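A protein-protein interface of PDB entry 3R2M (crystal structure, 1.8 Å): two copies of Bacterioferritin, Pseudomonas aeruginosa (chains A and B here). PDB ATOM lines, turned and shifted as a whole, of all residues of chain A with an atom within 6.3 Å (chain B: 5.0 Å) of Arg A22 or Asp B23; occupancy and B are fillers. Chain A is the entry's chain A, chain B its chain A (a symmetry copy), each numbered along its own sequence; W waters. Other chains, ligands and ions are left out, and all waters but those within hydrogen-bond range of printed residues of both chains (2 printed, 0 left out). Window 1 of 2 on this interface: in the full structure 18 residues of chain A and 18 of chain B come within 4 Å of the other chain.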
ATOM      1  N   GLY A  17     -29.811 -28.576  25.821  1.00  0.00           N
ATOM      2  CA  GLY A  17     -29.613 -27.140  25.952  1.00  0.00           C
ATOM      3  C   GLY A  17     -28.338 -26.786  26.738  1.00  0.00           C
ATOM      4  O   GLY A  17     -27.662 -25.821  26.416  1.00  0.00           O
ATOM      5  N   GLU A  18     -28.030 -27.553  27.782  1.00  0.00           N
ATOM      6  CA  GLU A  18     -26.850 -27.281  28.616  1.00  0.00           C
ATOM      7  C   GLU A  18     -25.576 -27.654  27.880  1.00  0.00           C
ATOM      8  O   GLU A  18     -24.556 -26.961  27.989  1.00  0.00           O
ATOM      9  CB  GLU A  18     -26.913 -28.079  29.939  1.00  0.00           C
ATOM     10  CG  GLU A  18     -28.090 -27.729  30.820  1.00  0.00           C
ATOM     11  CD  GLU A  18     -28.109 -26.287  31.220  1.00  0.00           C
ATOM     12  OE1 GLU A  18     -27.048 -25.756  31.563  1.00  0.00           O
ATOM     13  OE2 GLU A  18     -29.189 -25.668  31.195  1.00  0.00           O
ATOM     14  N   LEU A  19     -25.614 -28.755  27.140  1.00  0.00           N
ATOM     15  CA  LEU A  19     -24.474 -29.148  26.324  1.00  0.00           C
ATOM     16  C   LEU A  19     -24.176 -28.045  25.290  1.00  0.00           C
ATOM     17  O   LEU A  19     -23.016 -27.723  25.027  1.00  0.00           O
ATOM     18  CB  LEU A  19     -24.742 -30.486  25.608  1.00  0.00           C
ATOM     19  CG  LEU A  19     -24.935 -31.704  26.525  1.00  0.00           C
ATOM     20  CD1 LEU A  19     -25.436 -32.904  25.699  1.00  0.00           C
ATOM     21  CD2 LEU A  19     -23.601 -32.072  27.279  1.00  0.00           C
ATOM     22  N   ALA A  20     -25.219 -27.464  24.700  1.00  0.00           N
ATOM     23  CA  ALA A  20     -25.026 -26.321  23.813  1.00  0.00           C
ATOM     24  C   ALA A  20     -24.459 -25.072  24.508  1.00  0.00           C
ATOM     25  O   ALA A  20     -23.583 -24.399  23.953  1.00  0.00           O
ATOM     26  CB  ALA A  20     -26.380 -25.941  23.099  1.00  0.00           C
ATOM     27  N   ALA A  21     -25.004 -24.715  25.672  1.00  0.00           N
ATOM     28  CA  ALA A  21     -24.487 -23.564  26.445  1.00  0.00           C
ATOM     29  C   ALA A  21     -22.979 -23.740  26.706  1.00  0.00           C
ATOM     30  O   ALA A  21     -22.187 -22.806  26.484  1.00  0.00           O
ATOM     31  CB  ALA A  21     -25.221 -23.438  27.765  1.00  0.00           C
ATOM     32  N   ARG A  22     -22.604 -24.935  27.191  1.00  0.00           N
ATOM     33  CA  ARG A  22     -21.178 -25.313  27.368  1.00  0.00           C
ATOM     34  C   ARG A  22     -20.366 -25.001  26.096  1.00  0.00           C
ATOM     35  O   ARG A  22     -19.325 -24.351  26.134  1.00  0.00           O
ATOM     36  CB  ARG A  22     -21.094 -26.807  27.690  1.00  0.00           C
ATOM     37  CG  ARG A  22     -19.681 -27.425  27.562  1.00  0.00           C
ATOM     38  CD  ARG A  22     -19.759 -28.984  27.437  1.00  0.00           C
ATOM     39  NE  ARG A  22     -20.493 -29.390  26.224  1.00  0.00           N
ATOM     40  CZ  ARG A  22     -20.546 -30.631  25.742  1.00  0.00           C
ATOM     41  NH1 ARG A  22     -19.909 -31.636  26.353  1.00  0.00           N
ATOM     42  NH2 ARG A  22     -21.234 -30.867  24.632  1.00  0.00           N
ATOM     43  N   ASP A  23     -20.851 -25.451  24.949  1.00  0.00           N
ATOM     44  CA  ASP A  23     -20.129 -25.248  23.692  1.00  0.00           C
ATOM     45  C   ASP A  23     -20.128 -23.828  23.161  1.00  0.00           C
ATOM     46  O   ASP A  23     -19.129 -23.392  22.554  1.00  0.00           O
ATOM     47  CB  ASP A  23     -20.637 -26.239  22.625  1.00  0.00           C
ATOM     48  CG  ASP A  23     -20.144 -27.644  22.900  1.00  0.00           C
ATOM     49  OD1 ASP A  23     -19.164 -27.751  23.678  1.00  0.00           O
ATOM     50  OD2 ASP A  23     -20.702 -28.612  22.360  1.00  0.00           O
ATOM     51  N   GLN A  24     -21.166 -23.066  23.447  1.00  0.00           N
ATOM     52  CA  GLN A  24     -21.155 -21.669  23.032  1.00  0.00           C
ATOM     53  C   GLN A  24     -20.156 -20.868  23.889  1.00  0.00           C
ATOM     54  O   GLN A  24     -19.454 -19.996  23.403  1.00  0.00           O
ATOM     55  CB  GLN A  24     -22.554 -21.061  23.113  1.00  0.00           C
ATOM     56  CG  GLN A  24     -22.624 -19.634  22.610  1.00  0.00           C
ATOM     57  CD  GLN A  24     -24.063 -19.221  22.296  1.00  0.00           C
ATOM     58  OE1 GLN A  24     -24.725 -19.892  21.520  1.00  0.00           O
ATOM     59  NE2 GLN A  24     -24.556 -18.147  22.934  1.00  0.00           N
ATOM     60  N   TYR A  25     -20.061 -21.189  25.179  1.00  0.00           N
ATOM     61  CA  TYR A  25     -19.044 -20.545  26.015  1.00  0.00           C
ATOM     62  C   TYR A  25     -17.631 -21.040  25.649  1.00  0.00           C
ATOM     63  O   TYR A  25     -16.672 -20.283  25.776  1.00  0.00           O
ATOM     64  CB  TYR A  25     -19.332 -20.857  27.486  1.00  0.00           C
ATOM     65  CG  TYR A  25     -20.515 -20.084  28.059  1.00  0.00           C
ATOM     66  CD1 TYR A  25     -20.644 -18.715  27.831  1.00  0.00           C
ATOM     67  CD2 TYR A  25     -21.457 -20.705  28.859  1.00  0.00           C
ATOM     68  CE1 TYR A  25     -21.694 -17.982  28.379  1.00  0.00           C
ATOM     69  CE2 TYR A  25     -22.516 -19.990  29.395  1.00  0.00           C
ATOM     70  CZ  TYR A  25     -22.621 -18.617  29.153  1.00  0.00           C
ATOM     71  OH  TYR A  25     -23.644 -17.864  29.700  1.00  0.00           O
ATOM     72  N   PHE A  26     -17.517 -22.287  25.172  1.00  0.00           N
ATOM     73  CA  PHE A  26     -16.230 -22.849  24.687  1.00  0.00           C
ATOM     74  C   PHE A  26     -15.711 -21.935  23.556  1.00  0.00           C
ATOM     75  O   PHE A  26     -14.611 -21.376  23.617  1.00  0.00           O
ATOM     76  CB  PHE A  26     -16.452 -24.296  24.173  1.00  0.00           C
ATOM     77  CG  PHE A  26     -15.197 -25.181  24.088  1.00  0.00           C
ATOM     78  CD1 PHE A  26     -13.909 -24.688  24.311  1.00  0.00           C
ATOM     79  CD2 PHE A  26     -15.335 -26.526  23.761  1.00  0.00           C
ATOM     80  CE1 PHE A  26     -12.810 -25.518  24.226  1.00  0.00           C
ATOM     81  CE2 PHE A  26     -14.234 -27.372  23.675  1.00  0.00           C
ATOM     82  CZ  PHE A  26     -12.964 -26.869  23.929  1.00  0.00           C
ATOM     83  N   ILE A  27     -16.517 -21.745  22.524  1.00  0.00           N
ATOM     84  CA  ILE A  27     -16.057 -20.933  21.407  1.00  0.00           C
ATOM     85  C   ILE A  27     -15.914 -19.463  21.796  1.00  0.00           C
ATOM     86  O   ILE A  27     -14.889 -18.847  21.451  1.00  0.00           O
ATOM     87  CB  ILE A  27     -16.944 -21.126  20.114  1.00  0.00           C
ATOM     88  CG1 ILE A  27     -16.411 -20.269  18.954  1.00  0.00           C
ATOM     89  CG2 ILE A  27     -18.419 -20.727  20.377  1.00  0.00           C
ATOM     90  CD1 ILE A  27     -15.000 -20.593  18.519  1.00  0.00           C
ATOM     91  N   GLU A  47     -17.574 -20.183  32.947  1.00  0.00           N
ATOM     92  CA  GLU A  47     -18.970 -20.510  32.682  1.00  0.00           C
ATOM     93  C   GLU A  47     -19.110 -21.835  31.895  1.00  0.00           C
ATOM     94  O   GLU A  47     -20.024 -22.600  32.154  1.00  0.00           O
ATOM     95  CB  GLU A  47     -19.672 -19.397  31.923  1.00  0.00           C
ATOM     96  CG  GLU A  47     -19.628 -18.032  32.584  1.00  0.00           C
ATOM     97  CD  GLU A  47     -20.369 -17.976  33.899  1.00  0.00           C
ATOM     98  OE1 GLU A  47     -21.598 -17.732  33.866  1.00  0.00           O
ATOM     99  OE2 GLU A  47     -19.722 -18.156  34.962  1.00  0.00           O
ATOM    100  N   MET A  48     -18.205 -22.099  30.952  1.00  0.00           N
ATOM    101  CA  MET A  48     -18.166 -23.399  30.256  1.00  0.00           C
ATOM    102  C   MET A  48     -18.075 -24.549  31.243  1.00  0.00           C
ATOM    103  O   MET A  48     -18.830 -25.535  31.151  1.00  0.00           O
ATOM    104  CB  MET A  48     -16.965 -23.483  29.299  1.00  0.00           C
ATOM    105  CG  MET A  48     -16.900 -24.793  28.544  1.00  0.00           C
ATOM    106  SD  MET A  48     -15.456 -24.959  27.477  1.00  0.00           S
ATOM    107  CE  MET A  48     -14.134 -25.193  28.685  1.00  0.00           C
ATOM    108  N   GLU A  49     -17.186 -24.443  32.226  1.00  0.00           N
ATOM    109  CA  GLU A  49     -17.101 -25.500  33.263  1.00  0.00           C
ATOM    110  C   GLU A  49     -18.408 -25.636  34.058  1.00  0.00           C
ATOM    111  O   GLU A  49     -18.855 -26.747  34.351  1.00  0.00           O
ATOM    112  CB  GLU A  49     -15.904 -25.220  34.214  1.00  0.00           C
ATOM    113  CG  GLU A  49     -14.574 -25.269  33.450  1.00  0.00           C
ATOM    114  CD  GLU A  49     -13.356 -24.736  34.225  1.00  0.00           C
ATOM    115  OE1 GLU A  49     -13.513 -23.981  35.212  1.00  0.00           O
ATOM    116  OE2 GLU A  49     -12.221 -25.066  33.810  1.00  0.00           O
ATOM    117  N   GLU A  51     -21.528 -24.902  33.008  1.00  0.00           N
ATOM    118  CA  GLU A  51     -22.533 -25.561  32.185  1.00  0.00           C
ATOM    119  C   GLU A  51     -22.212 -27.034  32.038  1.00  0.00           C
ATOM    120  O   GLU A  51     -23.111 -27.848  31.923  1.00  0.00           O
ATOM    121  CB  GLU A  51     -22.618 -24.961  30.777  1.00  0.00           C
ATOM    122  CG  GLU A  51     -22.869 -23.485  30.738  1.00  0.00           C
ATOM    123  CD  GLU A  51     -24.204 -23.061  31.345  1.00  0.00           C
ATOM    124  OE1 GLU A  51     -24.989 -23.903  31.759  1.00  0.00           O
ATOM    125  OE2 GLU A  51     -24.461 -21.853  31.384  1.00  0.00           O
ATOM    126  N   THR A  52     -20.932 -27.393  32.014  1.00  0.00           N
ATOM    127  CA  THR A  52     -20.565 -28.817  31.964  1.00  0.00           C
ATOM    128  C   THR A  52     -21.092 -29.510  33.220  1.00  0.00           C
ATOM    129  O   THR A  52     -21.656 -30.614  33.168  1.00  0.00           O
ATOM    130  CB  THR A  52     -19.038 -29.018  31.807  1.00  0.00           C
ATOM    131  OG1 THR A  52     -18.590 -28.367  30.610  1.00  0.00           O
ATOM    132  CG2 THR A  52     -18.684 -30.505  31.682  1.00  0.00           C
ATOM    133  N   ALA A  55     -24.928 -29.833  32.887  1.00  0.00           N
ATOM    134  CA  ALA A  55     -25.220 -30.976  32.023  1.00  0.00           C
ATOM    135  C   ALA A  55     -24.980 -32.289  32.761  1.00  0.00           C
ATOM    136  O   ALA A  55     -25.795 -33.217  32.701  1.00  0.00           O
ATOM    137  CB  ALA A  55     -24.361 -30.912  30.792  1.00  0.00           C
ATOM    138  N   MET A  71     -27.581 -36.932  23.834  1.00  0.00           N
ATOM    139  CA  MET A  71     -26.278 -36.261  23.918  1.00  0.00           C
ATOM    140  C   MET A  71     -26.013 -35.277  22.776  1.00  0.00           C
ATOM    141  O   MET A  71     -24.957 -34.638  22.722  1.00  0.00           O
ATOM    142  CB  MET A  71     -25.155 -37.310  23.998  1.00  0.00           C
ATOM    143  CG  MET A  71     -25.234 -38.204  25.247  1.00  0.00           C
ATOM    144  SD  MET A  71     -25.047 -37.222  26.772  1.00  0.00           S
ATOM    145  CE  MET A  71     -23.408 -36.543  26.586  1.00  0.00           C
ATOM    146  N   PRO A  73     -25.950 -31.864  21.242  1.00  0.00           N
ATOM    147  CA  PRO A  73     -26.237 -30.508  21.723  1.00  0.00           C
ATOM    148  C   PRO A  73     -27.173 -29.736  20.787  1.00  0.00           C
ATOM    149  O   PRO A  73     -27.137 -29.954  19.575  1.00  0.00           O
ATOM    150  CB  PRO A  73     -24.860 -29.812  21.705  1.00  0.00           C
ATOM    151  CG  PRO A  73     -23.851 -30.940  21.693  1.00  0.00           C
ATOM    152  CD  PRO A  73     -24.526 -32.040  20.894  1.00  0.00           C
ATOM    153  N   LEU A  92     -29.263 -16.760  25.134  1.00  0.00           N
ATOM    154  CA  LEU A  92     -29.245 -18.181  25.507  1.00  0.00           C
ATOM    155  C   LEU A  92     -29.616 -18.401  26.975  1.00  0.00           C
ATOM    156  O   LEU A  92     -30.399 -19.288  27.288  1.00  0.00           O
ATOM    157  CB  LEU A  92     -27.846 -18.796  25.215  1.00  0.00           C
ATOM    158  CG  LEU A  92     -27.739 -20.322  25.429  1.00  0.00           C
ATOM    159  CD1 LEU A  92     -28.999 -21.052  24.952  1.00  0.00           C
ATOM    160  CD2 LEU A  92     -26.557 -20.910  24.702  1.00  0.00           C
ATOM    161  N   LEU B  19     -14.843 -33.186  19.639  1.00  0.00           N
ATOM    162  CA  LEU B  19     -15.995 -32.795  20.439  1.00  0.00           C
ATOM    163  C   LEU B  19     -16.928 -34.007  20.624  1.00  0.00           C
ATOM    164  O   LEU B  19     -17.474 -34.224  21.707  1.00  0.00           O
ATOM    165  CB  LEU B  19     -16.759 -31.633  19.776  1.00  0.00           C
ATOM    166  CG  LEU B  19     -15.981 -30.315  19.641  1.00  0.00           C
ATOM    167  CD1 LEU B  19     -16.766 -29.335  18.749  1.00  0.00           C
ATOM    168  CD2 LEU B  19     -15.694 -29.670  21.051  1.00  0.00           C
ATOM    169  N   ALA B  20     -17.118 -34.797  19.569  1.00  0.00           N
ATOM    170  CA  ALA B  20     -17.876 -36.037  19.699  1.00  0.00           C
ATOM    171  C   ALA B  20     -17.230 -37.079  20.626  1.00  0.00           C
ATOM    172  O   ALA B  20     -17.927 -37.722  21.419  1.00  0.00           O
ATOM    173  CB  ALA B  20     -18.118 -36.689  18.284  1.00  0.00           C
ATOM    174  N   ALA B  21     -15.923 -37.306  20.479  1.00  0.00           N
ATOM    175  CA  ALA B  21     -15.199 -38.246  21.363  1.00  0.00           C
ATOM    176  C   ALA B  21     -15.407 -37.848  22.837  1.00  0.00           C
ATOM    177  O   ALA B  21     -15.734 -38.703  23.681  1.00  0.00           O
ATOM    178  CB  ALA B  21     -13.718 -38.244  21.040  1.00  0.00           C
ATOM    179  N   ARG B  22     -15.200 -36.553  23.130  1.00  0.00           N
ATOM    180  CA  ARG B  22     -15.489 -35.981  24.470  1.00  0.00           C
ATOM    181  C   ARG B  22     -16.894 -36.395  24.951  1.00  0.00           C
ATOM    182  O   ARG B  22     -17.080 -36.899  26.055  1.00  0.00           O
ATOM    183  CB  ARG B  22     -15.389 -34.456  24.394  1.00  0.00           C
ATOM    184  CG  ARG B  22     -15.993 -33.701  25.602  1.00  0.00           C
ATOM    185  CD  ARG B  22     -16.279 -32.204  25.242  1.00  0.00           C
ATOM    186  NE  ARG B  22     -17.269 -32.092  24.153  1.00  0.00           N
ATOM    187  CZ  ARG B  22     -17.861 -30.960  23.773  1.00  0.00           C
ATOM    188  NH1 ARG B  22     -17.587 -29.800  24.380  1.00  0.00           N
ATOM    189  NH2 ARG B  22     -18.745 -30.993  22.784  1.00  0.00           N
ATOM    190  N   ASP B  23     -17.898 -36.198  24.109  1.00  0.00           N
ATOM    191  CA  ASP B  23     -19.275 -36.513  24.491  1.00  0.00           C
ATOM    192  C   ASP B  23     -19.608 -37.990  24.580  1.00  0.00           C
ATOM    193  O   ASP B  23     -20.420 -38.395  25.437  1.00  0.00           O
ATOM    194  CB  ASP B  23     -20.263 -35.777  23.562  1.00  0.00           C
ATOM    195  CG  ASP B  23     -20.314 -34.298  23.877  1.00  0.00           C
ATOM    196  OD1 ASP B  23     -19.871 -33.947  24.999  1.00  0.00           O
ATOM    197  OD2 ASP B  23     -20.783 -33.504  23.046  1.00  0.00           O
ATOM    198  N   GLN B  24     -18.944 -38.816  23.794  1.00  0.00           N
ATOM    199  CA  GLN B  24     -19.172 -40.250  23.920  1.00  0.00           C
ATOM    200  C   GLN B  24     -18.549 -40.774  25.228  1.00  0.00           C
ATOM    201  O   GLN B  24     -19.108 -41.622  25.906  1.00  0.00           O
ATOM    202  CB  GLN B  24     -18.617 -41.001  22.711  1.00  0.00           C
ATOM    203  CG  GLN B  24     -18.902 -42.489  22.741  1.00  0.00           C
ATOM    204  CD  GLN B  24     -18.735 -43.119  21.358  1.00  0.00           C
ATOM    205  OE1 GLN B  24     -19.362 -42.668  20.412  1.00  0.00           O
ATOM    206  NE2 GLN B  24     -17.857 -44.127  21.234  1.00  0.00           N
ATOM    207  N   TYR B  25     -17.391 -40.239  25.611  1.00  0.00           N
ATOM    208  CA  TYR B  25     -16.812 -40.611  26.906  1.00  0.00           C
ATOM    209  C   TYR B  25     -17.628 -40.014  28.070  1.00  0.00           C
ATOM    210  O   TYR B  25     -17.692 -40.619  29.138  1.00  0.00           O
ATOM    211  CB  TYR B  25     -15.370 -40.103  26.977  1.00  0.00           C
ATOM    212  CG  TYR B  25     -14.390 -40.910  26.132  1.00  0.00           C
ATOM    213  CD1 TYR B  25     -14.404 -42.303  26.170  1.00  0.00           C
ATOM    214  CD2 TYR B  25     -13.433 -40.287  25.351  1.00  0.00           C
ATOM    215  CE1 TYR B  25     -13.491 -43.061  25.438  1.00  0.00           C
ATOM    216  CE2 TYR B  25     -12.533 -41.029  24.605  1.00  0.00           C
ATOM    217  CZ  TYR B  25     -12.566 -42.426  24.662  1.00  0.00           C
ATOM    218  OH  TYR B  25     -11.659 -43.198  23.959  1.00  0.00           O
ATOM    219  N   PHE B  26     -18.265 -38.857  27.849  1.00  0.00           N
ATOM    220  CA  PHE B  26     -19.166 -38.229  28.850  1.00  0.00           C
ATOM    221  C   PHE B  26     -20.278 -39.244  29.188  1.00  0.00           C
ATOM    222  O   PHE B  26     -20.471 -39.648  30.339  1.00  0.00           O
ATOM    223  CB  PHE B  26     -19.764 -36.922  28.267  1.00  0.00           C
ATOM    224  CG  PHE B  26     -20.315 -35.917  29.293  1.00  0.00           C
ATOM    225  CD1 PHE B  26     -20.416 -36.207  30.655  1.00  0.00           C
ATOM    226  CD2 PHE B  26     -20.749 -34.669  28.856  1.00  0.00           C
ATOM    227  CE1 PHE B  26     -20.914 -35.275  31.542  1.00  0.00           C
ATOM    228  CE2 PHE B  26     -21.252 -33.721  29.742  1.00  0.00           C
ATOM    229  CZ  PHE B  26     -21.316 -34.019  31.097  1.00  0.00           C
ATOM    230  N   ILE B  27     -21.003 -39.695  28.177  1.00  0.00           N
ATOM    231  CA  ILE B  27     -22.098 -40.615  28.444  1.00  0.00           C
ATOM    232  C   ILE B  27     -21.592 -41.974  28.923  1.00  0.00           C
ATOM    233  O   ILE B  27     -22.140 -42.510  29.904  1.00  0.00           O
ATOM    234  CB  ILE B  27     -23.093 -40.743  27.225  1.00  0.00           C
ATOM    235  CG1 ILE B  27     -24.244 -41.706  27.559  1.00  0.00           C
ATOM    236  CG2 ILE B  27     -22.370 -41.271  25.959  1.00  0.00           C
ATOM    237  CD1 ILE B  27     -25.105 -41.288  28.730  1.00  0.00           C
ATOM    238  N   PRO B  73     -20.724 -31.138  17.236  1.00  0.00           N
ATOM    239  CA  PRO B  73     -20.020 -32.422  17.311  1.00  0.00           C
ATOM    240  C   PRO B  73     -20.545 -33.443  16.297  1.00  0.00           C
ATOM    241  O   PRO B  73     -21.733 -33.421  15.971  1.00  0.00           O
ATOM    242  CB  PRO B  73     -20.351 -32.940  18.727  1.00  0.00           C
ATOM    243  CG  PRO B  73     -20.790 -31.715  19.499  1.00  0.00           C
ATOM    244  CD  PRO B  73     -21.488 -30.848  18.466  1.00  0.00           C
ATOM    245  N   ILE B  76     -22.520 -39.371  17.946  1.00  0.00           N
ATOM    246  CA  ILE B  76     -21.888 -40.401  18.742  1.00  0.00           C
ATOM    247  C   ILE B  76     -22.710 -41.685  18.678  1.00  0.00           C
ATOM    248  O   ILE B  76     -23.858 -41.678  18.216  1.00  0.00           O
ATOM    249  CB  ILE B  76     -21.693 -39.942  20.216  1.00  0.00           C
ATOM    250  CG1 ILE B  76     -23.043 -39.671  20.880  1.00  0.00           C
ATOM    251  CG2 ILE B  76     -20.774 -38.685  20.253  1.00  0.00           C
ATOM    252  CD1 ILE B  76     -22.950 -39.628  22.435  1.00  0.00           C
HETATM  253  O   HOH W   1     -22.412 -34.835  21.493  1.00  0.00           O
HETATM  254  O   HOH W   2     -16.140 -28.512  26.658  1.00  0.00           O
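NH1 of Arg A22 is in salt-bridge range of OD1 of Asp B23 (2.7 Å). The side-chain carboxylate (OD1) of Asp A23 lies within salt-bridge range of the guanidinium group (NH1) of Arg B22 (2.7 Å). The guanidinium group of Arg A22 lies close to the guanidinium group of Arg B22, 3.1 Å away.
The guanidinium group (NE) of Arg A22 sits at hydrogen-bond distance from the backbone carbonyl oxygen (O) of Leu A19 (3.3 Å). O of Met A48 sits at hydrogen-bond distance from OG1 of Thr A52, at 2.9 Å. The guanidinium group of Arg B22 lies within salt-bridge range of the side-chain carboxylate of Asp B23 (3.2 Å). O of Leu B19 lies within hydrogen-bond range of NE of Arg B22, 3.3 Å away. NH2 of Arg A22 lies within salt-bridge range of OD2 of Asp A23 (3.2 Å).
Among the printed residues, merely in contact across the chains: Met A71 with Ile B76, Met A71 with Asp B23, Phe A26 with Leu B19, Leu A19 with Phe B26, Pro A73 with Pro B73, Met A71 with Ile B27, Met A71 with Phe B26 and Thr A52 with Phe B26.
Asp B23 touches just these residues of chain A: Arg A22 (2.7 Å) and Met A71 (3.7 Å). Printed residues of chain A within 4 Å of Ile B27: Met A71 (3.9 Å). Of the printed residues of chain B, Phe A26 touches Leu B19 (3.8 Å). Printed residues of chain A within 4 Å of Arg B22: Arg A22 (3.1 Å) and Asp A23 (2.7 Å).
Of the 11 printed residues of chain B, 7 touch a printed residue of chain A. Printed residues of chain A that touch a printed residue of chain B: Leu A19, Arg A22, Asp A23, Phe A26, Thr A52, Met A71 and Pro A73. Hydrophobic or aromatic side chains of chain A within 4 Å of the printed part of chain B: Leu A19, Phe A26, Met A71 and Pro A73.
Leu A19 touches Phe B26, and with the chains exchanged Phe A26 touches Leu B19. Arg A22 touches its own counterpart, Arg B22. Arg A22 touches Asp B23, and with the chains exchanged Asp A23 touches Arg B22. Pro B73 touches its own counterpart, Pro A73. 10 positions are printed for both chains. Of the 11 pairs that touch across the chains among the printed residues, 6 have their exchanged pair printed and touching as well.
Water W1 bridges OD2 of Asp B23 (2.6 Å) and O of Met A71 (2.8 Å). Water W2 bridges NH1 of Arg B22 (3.0 Å) and SD of Met A48 (3.7 Å).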
